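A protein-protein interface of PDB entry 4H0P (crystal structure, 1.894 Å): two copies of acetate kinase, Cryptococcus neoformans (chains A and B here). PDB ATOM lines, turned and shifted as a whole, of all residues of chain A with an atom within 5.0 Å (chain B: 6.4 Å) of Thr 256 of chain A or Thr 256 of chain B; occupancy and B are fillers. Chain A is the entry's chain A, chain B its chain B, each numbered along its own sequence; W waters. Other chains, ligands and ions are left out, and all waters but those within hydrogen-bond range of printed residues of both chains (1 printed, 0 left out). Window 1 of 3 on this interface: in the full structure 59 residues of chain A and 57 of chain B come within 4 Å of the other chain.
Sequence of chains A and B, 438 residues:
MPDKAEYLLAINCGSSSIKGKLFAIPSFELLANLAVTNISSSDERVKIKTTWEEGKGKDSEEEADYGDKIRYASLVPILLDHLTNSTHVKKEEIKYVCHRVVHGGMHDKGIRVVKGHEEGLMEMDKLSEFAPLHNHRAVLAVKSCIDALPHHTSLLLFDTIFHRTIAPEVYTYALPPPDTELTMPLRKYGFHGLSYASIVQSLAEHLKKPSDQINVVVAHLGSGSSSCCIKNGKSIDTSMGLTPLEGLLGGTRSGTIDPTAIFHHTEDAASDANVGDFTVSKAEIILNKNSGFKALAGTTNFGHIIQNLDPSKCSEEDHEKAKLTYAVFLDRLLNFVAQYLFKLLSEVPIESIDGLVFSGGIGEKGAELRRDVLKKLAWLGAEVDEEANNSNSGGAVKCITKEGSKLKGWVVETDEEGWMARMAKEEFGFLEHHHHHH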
ATOM      1  N   LEU A 245      31.131  15.923  -6.150  1.00  0.00           N
ATOM      2  CA  LEU A 245      31.287  15.325  -7.476  1.00  0.00           C
ATOM      3  C   LEU A 245      31.688  16.385  -8.516  1.00  0.00           C
ATOM      4  O   LEU A 245      32.525  16.146  -9.396  1.00  0.00           O
ATOM      5  CB  LEU A 245      29.976  14.654  -7.877  1.00  0.00           C
ATOM      6  CG  LEU A 245      29.973  14.167  -9.321  1.00  0.00           C
ATOM      7  CD1 LEU A 245      31.092  13.134  -9.471  1.00  0.00           C
ATOM      8  CD2 LEU A 245      28.641  13.590  -9.679  1.00  0.00           C
ATOM      9  N   GLU A 246      31.095  17.567  -8.390  1.00  0.00           N
ATOM     10  CA  GLU A 246      31.226  18.630  -9.379  1.00  0.00           C
ATOM     11  C   GLU A 246      32.663  19.162  -9.421  1.00  0.00           C
ATOM     12  O   GLU A 246      33.379  19.145  -8.424  1.00  0.00           O
ATOM     13  CB  GLU A 246      30.210  19.747  -9.068  1.00  0.00           C
ATOM     14  CG  GLU A 246      30.186  20.918 -10.066  1.00  0.00           C
ATOM     15  CD  GLU A 246      29.001  21.862  -9.844  1.00  0.00           C
ATOM     16  OE1 GLU A 246      28.109  21.526  -9.028  1.00  0.00           O
ATOM     17  OE2 GLU A 246      28.959  22.941 -10.486  1.00  0.00           O
ATOM     18  N   GLY A 247      33.111  19.583 -10.600  1.00  0.00           N
ATOM     19  CA  GLY A 247      34.404  20.233 -10.700  1.00  0.00           C
ATOM     20  C   GLY A 247      35.452  19.312 -11.279  1.00  0.00           C
ATOM     21  O   GLY A 247      35.256  18.758 -12.353  1.00  0.00           O
ATOM     22  N   LEU A 248      36.560  19.140 -10.564  1.00  0.00           N
ATOM     23  CA  LEU A 248      37.633  18.277 -11.040  1.00  0.00           C
ATOM     24  C   LEU A 248      37.271  16.799 -10.942  1.00  0.00           C
ATOM     25  O   LEU A 248      36.550  16.376 -10.033  1.00  0.00           O
ATOM     26  CB  LEU A 248      38.901  18.519 -10.242  1.00  0.00           C
ATOM     27  CG  LEU A 248      39.397  19.947 -10.290  1.00  0.00           C
ATOM     28  CD1 LEU A 248      40.554  20.063  -9.326  1.00  0.00           C
ATOM     29  CD2 LEU A 248      39.861  20.192 -11.730  1.00  0.00           C
ATOM     30  N   SER A 254      33.721  11.503 -11.678  1.00  0.00           N
ATOM     31  CA  SER A 254      33.783  12.060 -13.037  1.00  0.00           C
ATOM     32  C   SER A 254      34.172  13.527 -13.065  1.00  0.00           C
ATOM     33  O   SER A 254      34.770  13.981 -14.024  1.00  0.00           O
ATOM     34  CB  SER A 254      32.417  11.936 -13.688  1.00  0.00           C
ATOM     35  OG  SER A 254      31.474  12.717 -12.990  1.00  0.00           O
ATOM     36  N   GLY A 255      33.813  14.278 -12.022  1.00  0.00           N
ATOM     37  CA  GLY A 255      33.930  15.719 -12.085  1.00  0.00           C
ATOM     38  C   GLY A 255      32.802  16.232 -12.973  1.00  0.00           C
ATOM     39  O   GLY A 255      31.852  15.495 -13.267  1.00  0.00           O
ATOM     40  N   THR A 256      32.902  17.486 -13.409  1.00  0.00           N
ATOM     41  CA  THR A 256      31.805  18.138 -14.129  1.00  0.00           C
ATOM     42  C   THR A 256      31.623  17.528 -15.516  1.00  0.00           C
ATOM     43  O   THR A 256      32.580  17.373 -16.263  1.00  0.00           O
ATOM     44  CB  THR A 256      32.065  19.654 -14.271  1.00  0.00           C
ATOM     45  OG1 THR A 256      31.926  20.277 -12.980  1.00  0.00           O
ATOM     46  CG2 THR A 256      31.068  20.287 -15.257  1.00  0.00           C
ATOM     47  N   ILE A 257      30.390  17.173 -15.849  1.00  0.00           N
ATOM     48  CA  ILE A 257      30.052  16.672 -17.171  1.00  0.00           C
ATOM     49  C   ILE A 257      28.641  17.166 -17.420  1.00  0.00           C
ATOM     50  O   ILE A 257      27.991  17.627 -16.488  1.00  0.00           O
ATOM     51  CB  ILE A 257      30.078  15.132 -17.221  1.00  0.00           C
ATOM     52  CG1 ILE A 257      29.251  14.564 -16.080  1.00  0.00           C
ATOM     53  CG2 ILE A 257      31.514  14.588 -17.124  1.00  0.00           C
ATOM     54  CD1 ILE A 257      28.751  13.162 -16.337  1.00  0.00           C
ATOM     55  N   ASP A 258      28.158  17.071 -18.657  1.00  0.00           N
ATOM     56  CA  ASP A 258      26.786  17.478 -18.969  1.00  0.00           C
ATOM     57  C   ASP A 258      25.822  16.732 -18.033  1.00  0.00           C
ATOM     58  O   ASP A 258      25.936  15.519 -17.871  1.00  0.00           O
ATOM     59  CB  ASP A 258      26.477  17.116 -20.422  1.00  0.00           C
ATOM     60  CG  ASP A 258      25.157  17.689 -20.913  1.00  0.00           C
ATOM     61  OD1 ASP A 258      24.081  17.394 -20.328  1.00  0.00           O
ATOM     62  OD2 ASP A 258      25.209  18.441 -21.901  1.00  0.00           O
ATOM     63  N   TYR B 173      35.276  12.970 -21.396  1.00  0.00           N
ATOM     64  CA  TYR B 173      34.517  12.849 -20.166  1.00  0.00           C
ATOM     65  C   TYR B 173      35.107  11.657 -19.431  1.00  0.00           C
ATOM     66  O   TYR B 173      35.345  10.619 -20.044  1.00  0.00           O
ATOM     67  CB  TYR B 173      33.060  12.532 -20.494  1.00  0.00           C
ATOM     68  CG  TYR B 173      32.175  13.745 -20.795  1.00  0.00           C
ATOM     69  CD1 TYR B 173      32.699  15.032 -20.861  1.00  0.00           C
ATOM     70  CD2 TYR B 173      30.819  13.590 -20.964  1.00  0.00           C
ATOM     71  CE1 TYR B 173      31.869  16.138 -21.114  1.00  0.00           C
ATOM     72  CE2 TYR B 173      29.978  14.680 -21.198  1.00  0.00           C
ATOM     73  CZ  TYR B 173      30.507  15.941 -21.266  1.00  0.00           C
ATOM     74  OH  TYR B 173      29.659  16.999 -21.502  1.00  0.00           O
ATOM     75  N   SER B 239      32.419  26.080 -24.398  1.00  0.00           N
ATOM     76  CA  SER B 239      31.741  25.952 -23.108  1.00  0.00           C
ATOM     77  C   SER B 239      30.672  24.873 -23.030  1.00  0.00           C
ATOM     78  O   SER B 239      30.321  24.417 -21.941  1.00  0.00           O
ATOM     79  CB  SER B 239      31.135  27.280 -22.672  1.00  0.00           C
ATOM     80  OG  SER B 239      30.216  27.734 -23.634  1.00  0.00           O
ATOM     81  N   LEU B 245      23.202  22.039 -23.192  1.00  0.00           N
ATOM     82  CA  LEU B 245      22.819  22.295 -21.811  1.00  0.00           C
ATOM     83  C   LEU B 245      24.018  22.762 -20.964  1.00  0.00           C
ATOM     84  O   LEU B 245      23.904  23.694 -20.157  1.00  0.00           O
ATOM     85  CB  LEU B 245      22.202  21.033 -21.207  1.00  0.00           C
ATOM     86  CG  LEU B 245      21.897  21.189 -19.721  1.00  0.00           C
ATOM     87  CD1 LEU B 245      20.848  22.260 -19.534  1.00  0.00           C
ATOM     88  CD2 LEU B 245      21.443  19.872 -19.127  1.00  0.00           C
ATOM     89  N   GLU B 246      25.168  22.120 -21.169  1.00  0.00           N
ATOM     90  CA  GLU B 246      26.391  22.364 -20.390  1.00  0.00           C
ATOM     91  C   GLU B 246      26.933  23.783 -20.599  1.00  0.00           C
ATOM     92  O   GLU B 246      26.784  24.382 -21.675  1.00  0.00           O
ATOM     93  CB  GLU B 246      27.468  21.298 -20.744  1.00  0.00           C
ATOM     94  CG  GLU B 246      28.762  21.313 -19.862  1.00  0.00           C
ATOM     95  CD  GLU B 246      29.771  20.190 -20.222  1.00  0.00           C
ATOM     96  OE1 GLU B 246      29.338  19.030 -20.417  1.00  0.00           O
ATOM     97  OE2 GLU B 246      30.997  20.459 -20.314  1.00  0.00           O
ATOM     98  N   GLY B 247      27.524  24.343 -19.559  1.00  0.00           N
ATOM     99  CA  GLY B 247      28.121  25.665 -19.662  1.00  0.00           C
ATOM    100  C   GLY B 247      27.240  26.769 -19.104  1.00  0.00           C
ATOM    101  O   GLY B 247      26.760  26.684 -17.973  1.00  0.00           O
ATOM    102  N   LEU B 248      27.015  27.807 -19.893  1.00  0.00           N
ATOM    103  CA  LEU B 248      26.266  28.965 -19.402  1.00  0.00           C
ATOM    104  C   LEU B 248      24.779  28.660 -19.310  1.00  0.00           C
ATOM    105  O   LEU B 248      24.215  27.974 -20.167  1.00  0.00           O
ATOM    106  CB  LEU B 248      26.461  30.159 -20.326  1.00  0.00           C
ATOM    107  CG  LEU B 248      27.901  30.638 -20.478  1.00  0.00           C
ATOM    108  CD1 LEU B 248      28.005  31.645 -21.640  1.00  0.00           C
ATOM    109  CD2 LEU B 248      28.279  31.299 -19.168  1.00  0.00           C
ATOM    110  N   LEU B 249      24.138  29.196 -18.277  1.00  0.00           N
ATOM    111  CA  LEU B 249      22.699  29.120 -18.172  1.00  0.00           C
ATOM    112  C   LEU B 249      22.119  29.942 -19.326  1.00  0.00           C
ATOM    113  O   LEU B 249      22.796  30.783 -19.909  1.00  0.00           O
ATOM    114  CB  LEU B 249      22.211  29.621 -16.803  1.00  0.00           C
ATOM    115  CG  LEU B 249      22.233  31.125 -16.517  1.00  0.00           C
ATOM    116  CD1 LEU B 249      21.463  31.480 -15.227  1.00  0.00           C
ATOM    117  CD2 LEU B 249      23.659  31.649 -16.442  1.00  0.00           C
ATOM    118  N   SER B 254      19.516  25.406 -17.428  1.00  0.00           N
ATOM    119  CA  SER B 254      20.217  25.574 -16.170  1.00  0.00           C
ATOM    120  C   SER B 254      21.673  25.910 -16.368  1.00  0.00           C
ATOM    121  O   SER B 254      22.297  26.500 -15.486  1.00  0.00           O
ATOM    122  CB  SER B 254      20.138  24.278 -15.385  1.00  0.00           C
ATOM    123  OG  SER B 254      20.827  23.242 -16.073  1.00  0.00           O
ATOM    124  N   GLY B 255      22.249  25.486 -17.492  1.00  0.00           N
ATOM    125  CA  GLY B 255      23.700  25.519 -17.611  1.00  0.00           C
ATOM    126  C   GLY B 255      24.323  24.483 -16.680  1.00  0.00           C
ATOM    127  O   GLY B 255      23.621  23.616 -16.158  1.00  0.00           O
ATOM    128  N   THR B 256      25.632  24.580 -16.463  1.00  0.00           N
ATOM    129  CA  THR B 256      26.376  23.606 -15.652  1.00  0.00           C
ATOM    130  C   THR B 256      25.978  23.612 -14.169  1.00  0.00           C
ATOM    131  O   THR B 256      25.963  24.650 -13.502  1.00  0.00           O
ATOM    132  CB  THR B 256      27.899  23.822 -15.797  1.00  0.00           C
ATOM    133  OG1 THR B 256      28.297  23.435 -17.125  1.00  0.00           O
ATOM    134  CG2 THR B 256      28.669  22.989 -14.772  1.00  0.00           C
ATOM    135  N   ILE B 257      25.629  22.435 -13.664  1.00  0.00           N
ATOM    136  CA  ILE B 257      25.270  22.240 -12.256  1.00  0.00           C
ATOM    137  C   ILE B 257      25.773  20.833 -11.899  1.00  0.00           C
ATOM    138  O   ILE B 257      26.151  20.059 -12.792  1.00  0.00           O
ATOM    139  CB  ILE B 257      23.746  22.281 -12.041  1.00  0.00           C
ATOM    140  CG1 ILE B 257      23.081  21.226 -12.919  1.00  0.00           C
ATOM    141  CG2 ILE B 257      23.137  23.667 -12.322  1.00  0.00           C
ATOM    142  CD1 ILE B 257      21.602  21.070 -12.620  1.00  0.00           C
ATOM    143  N   ASP B 258      25.788  20.491 -10.612  1.00  0.00           N
ATOM    144  CA  ASP B 258      26.215  19.144 -10.179  1.00  0.00           C
ATOM    145  C   ASP B 258      25.368  18.112 -10.935  1.00  0.00           C
ATOM    146  O   ASP B 258      24.136  18.249 -11.006  1.00  0.00           O
ATOM    147  CB  ASP B 258      25.992  19.012  -8.664  1.00  0.00           C
ATOM    148  CG  ASP B 258      26.551  17.722  -8.087  1.00  0.00           C
ATOM    149  OD1 ASP B 258      26.168  16.635  -8.573  1.00  0.00           O
ATOM    150  OD2 ASP B 258      27.374  17.797  -7.136  1.00  0.00           O
ATOM    151  N   PRO B 259      26.018  17.110 -11.557  1.00  0.00           N
ATOM    152  CA  PRO B 259      25.225  16.144 -12.324  1.00  0.00           C
ATOM    153  C   PRO B 259      24.212  15.386 -11.470  1.00  0.00           C
ATOM    154  O   PRO B 259      23.295  14.840 -12.040  1.00  0.00           O
ATOM    155  CB  PRO B 259      26.268  15.157 -12.860  1.00  0.00           C
ATOM    156  CG  PRO B 259      27.550  15.901 -12.861  1.00  0.00           C
ATOM    157  CD  PRO B 259      27.472  16.924 -11.758  1.00  0.00           C
ATOM    158  N   ARG B 332      29.320  33.542 -14.513  1.00  0.00           N
ATOM    159  CA  ARG B 332      29.590  32.347 -15.317  1.00  0.00           C
ATOM    160  C   ARG B 332      30.266  32.705 -16.610  1.00  0.00           C
ATOM    161  O   ARG B 332      31.163  31.990 -17.056  1.00  0.00           O
ATOM    162  CB  ARG B 332      28.325  31.545 -15.615  1.00  0.00           C
ATOM    163  CG  ARG B 332      27.587  31.068 -14.363  1.00  0.00           C
ATOM    164  CD  ARG B 332      28.437  30.251 -13.381  1.00  0.00           C
ATOM    165  NE  ARG B 332      27.544  29.827 -12.305  1.00  0.00           N
ATOM    166  CZ  ARG B 332      27.205  30.582 -11.267  1.00  0.00           C
ATOM    167  NH1 ARG B 332      27.737  31.786 -11.123  1.00  0.00           N
ATOM    168  NH2 ARG B 332      26.337  30.131 -10.372  1.00  0.00           N
ATOM    169  N   PHE B 336      34.357  31.482 -18.148  1.00  0.00           N
ATOM    170  CA  PHE B 336      34.825  30.937 -19.429  1.00  0.00           C
ATOM    171  C   PHE B 336      35.734  31.888 -20.166  1.00  0.00           C
ATOM    172  O   PHE B 336      36.690  31.468 -20.830  1.00  0.00           O
ATOM    173  CB  PHE B 336      33.662  30.517 -20.328  1.00  0.00           C
ATOM    174  CG  PHE B 336      32.954  29.323 -19.822  1.00  0.00           C
ATOM    175  CD1 PHE B 336      33.547  28.076 -19.918  1.00  0.00           C
ATOM    176  CD2 PHE B 336      31.719  29.442 -19.194  1.00  0.00           C
ATOM    177  CE1 PHE B 336      32.902  26.947 -19.406  1.00  0.00           C
ATOM    178  CE2 PHE B 336      31.082  28.326 -18.675  1.00  0.00           C
ATOM    179  CZ  PHE B 336      31.681  27.076 -18.777  1.00  0.00           C
HETATM  180  O   HOH W   1      33.166  18.743 -18.647  1.00  0.00           O
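The side-chain carboxylate (OE1) of Glu 246 of chain B sits at hydrogen-bond distance from the backbone NH (N) of Asp 258 of chain A. The side-chain carboxylate (OE1) of Glu 246 of chain A lies within hydrogen-bond range of the backbone NH (N) of Asp 258 of chain B (3.0 Å). The side-chain hydroxyl of Tyr 173 of chain B sits at hydrogen-bond distance from the backbone NH of Asp 258 of chain A (3.2 Å).
The backbone NH of Gly 247 of chain B is in hydrogen-bond range of the side-chain hydroxyl of Thr 256 of chain B (2.7 Å). N of Gly 247 of chain A is in hydrogen-bond range of OG1 of Thr 256 of chain A (2.7 Å).
Among the printed residues, pairs that only touch across the chains: Ile 257 of chain A with Glu 246 of chain B, Thr 256 of chain A with Thr 256 of chain B, Glu 246 of chain A with Ile 257 of chain B, Asp 258 of chain A with Leu 245 of chain B, Ile 257 of chain A with Tyr 173 of chain B and Ile 257 of chain A with Pro 259 of chain B.
Leu 248 of chain A touches none of the printed residues of chain B. Printed residues of chain B within 4 Å of Ile 257 of chain A: Tyr 173, Glu 246 and Pro 259. Of the printed residues of chain B, Asp 258 of chain A touches Tyr 173, Leu 245 and Glu 246. Of the printed residues of chain A, Leu 245 of chain B touches Asp 258. Leu 249 of chain B touches none of the printed residues of chain A. Thr 256 of chain B touches one residue of chain A. The nearest printed residue of chain B that does not touch Asp 258 of chain A is Pro 259 of chain B (5.0 Å).
Of the 15 printed residues of chain B, 7 touch a printed residue of chain A. Printed residues of chain B that touch a printed residue of chain A: Tyr 173, Leu 245, Glu 246, Thr 256, Ile 257, Asp 258 and Pro 259. Hydrophobic or aromatic side chains of chain B within 4 Å of the printed part of chain A: Tyr 173, Leu 245 and Pro 259. Of the 9 printed residues of chain A, 4 touch a printed residue of chain B. Printed residues of chain A that touch a printed residue of chain B: Glu 246, Thr 256, Ile 257 and Asp 258. Among the printed residues, 9 pairs touch across the chains. Among the printed residues, no Asp or Glu carboxylate lies within 4 Å of a Lys or Arg side-chain nitrogen of the other chain.
Glu 246 of chain A touches Ile 257 of chain B, and with the chains exchanged Ile 257 of chain A touches Glu 246 of chain B. Glu 246 of chain A touches Asp 258 of chain B, and with the chains exchanged Asp 258 of chain A touches Glu 246 of chain B. Thr 256 of chain A touches its own counterpart, Thr 256 of chain B. Asp 258 of chain A touches Leu 245 of chain B, but with the chains exchanged Leu 245 of chain A does not touch Asp 258 of chain B (4.1 Å).
Water W1 lies within hydrogen-bond range of the backbone carbonyl oxygen (O) of Thr 256 of chain A (2.8 Å) and the side-chain carboxylate (OE2) of Glu 246 of chain B (3.2 Å).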
